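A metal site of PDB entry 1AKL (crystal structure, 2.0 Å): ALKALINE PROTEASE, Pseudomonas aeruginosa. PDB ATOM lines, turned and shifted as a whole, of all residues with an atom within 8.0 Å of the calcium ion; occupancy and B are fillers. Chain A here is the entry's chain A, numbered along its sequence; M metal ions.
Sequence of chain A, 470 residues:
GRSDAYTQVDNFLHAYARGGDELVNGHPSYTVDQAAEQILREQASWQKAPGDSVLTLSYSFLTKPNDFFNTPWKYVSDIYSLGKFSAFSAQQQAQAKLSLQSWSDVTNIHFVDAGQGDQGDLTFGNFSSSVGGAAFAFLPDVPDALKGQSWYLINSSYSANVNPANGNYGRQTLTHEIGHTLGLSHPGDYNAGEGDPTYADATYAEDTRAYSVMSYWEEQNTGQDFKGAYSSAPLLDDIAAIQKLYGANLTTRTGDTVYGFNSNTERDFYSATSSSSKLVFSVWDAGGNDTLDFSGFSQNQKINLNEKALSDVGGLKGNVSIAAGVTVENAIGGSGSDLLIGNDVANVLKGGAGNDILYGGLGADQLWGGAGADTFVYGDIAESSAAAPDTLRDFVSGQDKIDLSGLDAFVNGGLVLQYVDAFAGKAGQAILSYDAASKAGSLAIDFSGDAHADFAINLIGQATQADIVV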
ATOM      1  N   ALA A 386     -30.594 -18.996  31.760  1.00  0.00           N
ATOM      2  CA  ALA A 386     -31.329 -20.164  32.170  1.00  0.00           C
ATOM      3  C   ALA A 386     -31.825 -19.878  33.583  1.00  0.00           C
ATOM      4  O   ALA A 386     -32.876 -20.362  34.001  1.00  0.00           O
ATOM      5  CB  ALA A 386     -30.432 -21.380  32.165  1.00  0.00           C
ATOM      6  N   PHE A 423     -28.488 -32.814  26.838  1.00  0.00           N
ATOM      7  CA  PHE A 423     -27.212 -32.174  26.621  1.00  0.00           C
ATOM      8  C   PHE A 423     -26.124 -33.222  26.779  1.00  0.00           C
ATOM      9  O   PHE A 423     -26.101 -33.949  27.773  1.00  0.00           O
ATOM     10  CB  PHE A 423     -27.015 -31.004  27.588  1.00  0.00           C
ATOM     11  CG  PHE A 423     -27.896 -29.802  27.282  1.00  0.00           C
ATOM     12  CD1 PHE A 423     -28.386 -29.577  25.989  1.00  0.00           C
ATOM     13  CD2 PHE A 423     -28.225 -28.883  28.284  1.00  0.00           C
ATOM     14  CE1 PHE A 423     -29.184 -28.471  25.702  1.00  0.00           C
ATOM     15  CE2 PHE A 423     -29.017 -27.775  28.005  1.00  0.00           C
ATOM     16  CZ  PHE A 423     -29.503 -27.570  26.713  1.00  0.00           C
ATOM     17  N   LYS A 426     -21.637 -30.802  23.794  1.00  0.00           N
ATOM     18  CA  LYS A 426     -21.213 -30.175  22.563  1.00  0.00           C
ATOM     19  C   LYS A 426     -21.911 -28.812  22.532  1.00  0.00           C
ATOM     20  O   LYS A 426     -22.997 -28.672  23.110  1.00  0.00           O
ATOM     21  CB  LYS A 426     -21.630 -31.033  21.357  1.00  0.00           C
ATOM     22  CG  LYS A 426     -21.199 -30.462  20.015  1.00  0.00           C
ATOM     23  CD  LYS A 426     -19.721 -30.045  20.046  1.00  0.00           C
ATOM     24  CE  LYS A 426     -19.446 -28.871  19.108  1.00  0.00           C
ATOM     25  NZ  LYS A 426     -18.109 -28.235  19.352  1.00  0.00           N
ATOM     26  N   ILE A 445     -30.745 -23.875  25.332  1.00  0.00           N
ATOM     27  CA  ILE A 445     -29.609 -24.011  24.439  1.00  0.00           C
ATOM     28  C   ILE A 445     -28.327 -23.989  25.246  1.00  0.00           C
ATOM     29  O   ILE A 445     -28.198 -23.209  26.206  1.00  0.00           O
ATOM     30  CB  ILE A 445     -29.559 -22.864  23.416  1.00  0.00           C
ATOM     31  CG1 ILE A 445     -30.883 -22.770  22.657  1.00  0.00           C
ATOM     32  CG2 ILE A 445     -28.424 -23.107  22.441  1.00  0.00           C
ATOM     33  CD1 ILE A 445     -30.948 -21.643  21.666  1.00  0.00           C
ATOM     34  N   ASP A 446     -27.406 -24.871  24.891  1.00  0.00           N
ATOM     35  CA  ASP A 446     -26.126 -24.927  25.573  1.00  0.00           C
ATOM     36  C   ASP A 446     -25.087 -24.330  24.645  1.00  0.00           C
ATOM     37  O   ASP A 446     -24.598 -24.999  23.735  1.00  0.00           O
ATOM     38  CB  ASP A 446     -25.728 -26.373  25.904  1.00  0.00           C
ATOM     39  CG  ASP A 446     -24.368 -26.474  26.596  1.00  0.00           C
ATOM     40  OD1 ASP A 446     -23.855 -25.470  27.145  1.00  0.00           O
ATOM     41  OD2 ASP A 446     -23.810 -27.590  26.597  1.00  0.00           O
ATOM     42  N   PHE A 447     -24.762 -23.063  24.860  1.00  0.00           N
ATOM     43  CA  PHE A 447     -23.767 -22.398  24.032  1.00  0.00           C
ATOM     44  C   PHE A 447     -22.326 -22.775  24.428  1.00  0.00           C
ATOM     45  O   PHE A 447     -21.462 -22.910  23.572  1.00  0.00           O
ATOM     46  CB  PHE A 447     -23.979 -20.878  24.044  1.00  0.00           C
ATOM     47  CG  PHE A 447     -25.169 -20.414  23.242  1.00  0.00           C
ATOM     48  CD1 PHE A 447     -25.089 -20.320  21.854  1.00  0.00           C
ATOM     49  CD2 PHE A 447     -26.377 -20.112  23.860  1.00  0.00           C
ATOM     50  CE1 PHE A 447     -26.201 -19.941  21.098  1.00  0.00           C
ATOM     51  CE2 PHE A 447     -27.485 -19.721  23.112  1.00  0.00           C
ATOM     52  CZ  PHE A 447     -27.397 -19.636  21.731  1.00  0.00           C
ATOM     53  N   SER A 448     -22.102 -23.009  25.717  1.00  0.00           N
ATOM     54  CA  SER A 448     -20.765 -23.340  26.201  1.00  0.00           C
ATOM     55  C   SER A 448     -20.355 -24.809  26.058  1.00  0.00           C
ATOM     56  O   SER A 448     -19.270 -25.200  26.498  1.00  0.00           O
ATOM     57  CB  SER A 448     -20.598 -22.914  27.660  1.00  0.00           C
ATOM     58  OG  SER A 448     -21.375 -23.718  28.550  1.00  0.00           O
ATOM     59  N   GLY A 449     -21.260 -25.632  25.528  1.00  0.00           N
ATOM     60  CA  GLY A 449     -20.953 -27.050  25.366  1.00  0.00           C
ATOM     61  C   GLY A 449     -20.747 -27.880  26.638  1.00  0.00           C
ATOM     62  O   GLY A 449     -20.339 -29.031  26.533  1.00  0.00           O
ATOM     63  N   ASP A 450     -21.028 -27.330  27.821  1.00  0.00           N
ATOM     64  CA  ASP A 450     -20.835 -28.114  29.054  1.00  0.00           C
ATOM     65  C   ASP A 450     -22.075 -28.899  29.493  1.00  0.00           C
ATOM     66  O   ASP A 450     -22.330 -29.077  30.690  1.00  0.00           O
ATOM     67  CB  ASP A 450     -20.278 -27.253  30.210  1.00  0.00           C
ATOM     68  CG  ASP A 450     -21.249 -26.197  30.739  1.00  0.00           C
ATOM     69  OD1 ASP A 450     -22.471 -26.438  30.776  1.00  0.00           O
ATOM     70  OD2 ASP A 450     -20.775 -25.125  31.174  1.00  0.00           O
ATOM     71  N   ALA A 451     -22.875 -29.307  28.519  1.00  0.00           N
ATOM     72  CA  ALA A 451     -24.104 -30.059  28.773  1.00  0.00           C
ATOM     73  C   ALA A 451     -25.112 -29.366  29.695  1.00  0.00           C
ATOM     74  O   ALA A 451     -25.976 -30.020  30.258  1.00  0.00           O
ATOM     75  CB  ALA A 451     -23.754 -31.440  29.324  1.00  0.00           C
ATOM     76  N   HIS A 452     -24.993 -28.050  29.845  1.00  0.00           N
ATOM     77  CA  HIS A 452     -25.910 -27.273  30.688  1.00  0.00           C
ATOM     78  C   HIS A 452     -26.398 -26.073  29.895  1.00  0.00           C
ATOM     79  O   HIS A 452     -25.582 -25.369  29.282  1.00  0.00           O
ATOM     80  CB  HIS A 452     -25.212 -26.767  31.948  1.00  0.00           C
ATOM     81  CG  HIS A 452     -24.761 -27.844  32.875  1.00  0.00           C
ATOM     82  ND1 HIS A 452     -23.862 -27.628  33.902  1.00  0.00           N
ATOM     83  CD2 HIS A 452     -25.096 -29.158  32.952  1.00  0.00           C
ATOM     84  CE1 HIS A 452     -23.660 -28.747  34.558  1.00  0.00           C
ATOM     85  NE2 HIS A 452     -24.400 -29.693  33.999  1.00  0.00           N
ATOM     86  N   ALA A 453     -27.709 -25.822  29.928  1.00  0.00           N
ATOM     87  CA  ALA A 453     -28.306 -24.690  29.211  1.00  0.00           C
ATOM     88  C   ALA A 453     -27.782 -23.368  29.750  1.00  0.00           C
ATOM     89  O   ALA A 453     -27.578 -23.234  30.953  1.00  0.00           O
ATOM     90  CB  ALA A 453     -29.816 -24.739  29.299  1.00  0.00           C
ATOM     91  N   ASP A 454     -27.436 -22.463  28.850  1.00  0.00           N
ATOM     92  CA  ASP A 454     -26.943 -21.135  29.243  1.00  0.00           C
ATOM     93  C   ASP A 454     -28.057 -20.150  28.950  1.00  0.00           C
ATOM     94  O   ASP A 454     -28.196 -19.140  29.648  1.00  0.00           O
ATOM     95  CB  ASP A 454     -25.745 -20.727  28.394  1.00  0.00           C
ATOM     96  CG  ASP A 454     -24.611 -21.710  28.461  1.00  0.00           C
ATOM     97  OD1 ASP A 454     -24.598 -22.640  27.627  1.00  0.00           O
ATOM     98  OD2 ASP A 454     -23.727 -21.526  29.323  1.00  0.00           O
ATOM     99  N   PHE A 455     -28.827 -20.465  27.918  1.00  0.00           N
ATOM    100  CA  PHE A 455     -29.915 -19.628  27.427  1.00  0.00           C
ATOM    101  C   PHE A 455     -31.185 -20.471  27.445  1.00  0.00           C
ATOM    102  O   PHE A 455     -31.178 -21.616  26.974  1.00  0.00           O
ATOM    103  CB  PHE A 455     -29.535 -19.204  25.999  1.00  0.00           C
ATOM    104  CG  PHE A 455     -30.576 -18.391  25.279  1.00  0.00           C
ATOM    105  CD1 PHE A 455     -30.606 -17.004  25.405  1.00  0.00           C
ATOM    106  CD2 PHE A 455     -31.462 -18.995  24.388  1.00  0.00           C
ATOM    107  CE1 PHE A 455     -31.494 -16.255  24.652  1.00  0.00           C
ATOM    108  CE2 PHE A 455     -32.350 -18.247  23.635  1.00  0.00           C
ATOM    109  CZ  PHE A 455     -32.370 -16.877  23.770  1.00  0.00           C
HETATM  110 CA    CA M   1     -23.565 -24.257  29.527  1.00  0.00          CA
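The backbone NH (N) of Gly 449 sits close to the side-chain carboxylate (OD2) of Asp 446, 3.4 Å away. N of Ala 451 is in hydrogen-bond range of OD2 of Asp 446, 2.7 Å away. The side-chain carboxylate (OD1) of Asp 454 lies close to the backbone NH (N) of Phe 447, 2.8 Å away. The backbone carbonyl oxygen (O) of Ile 445 is in hydrogen-bond range of the backbone NH (N) of Asp 454 (2.9 Å). The backbone NH (N) of Ala 386 lies within hydrogen-bond range of the backbone carbonyl oxygen (O) of Asp 454, 3.2 Å away.
The calcium ion is bound by O of His 452 (2.3 Å), OG of Ser 448 (2.5 Å), OD1 of Asp 446 (2.7 Å), OD1 of Asp 454 (2.7 Å), OD1 of Asp 450 (2.7 Å) and OD2 of Asp 454 (2.7 Å).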
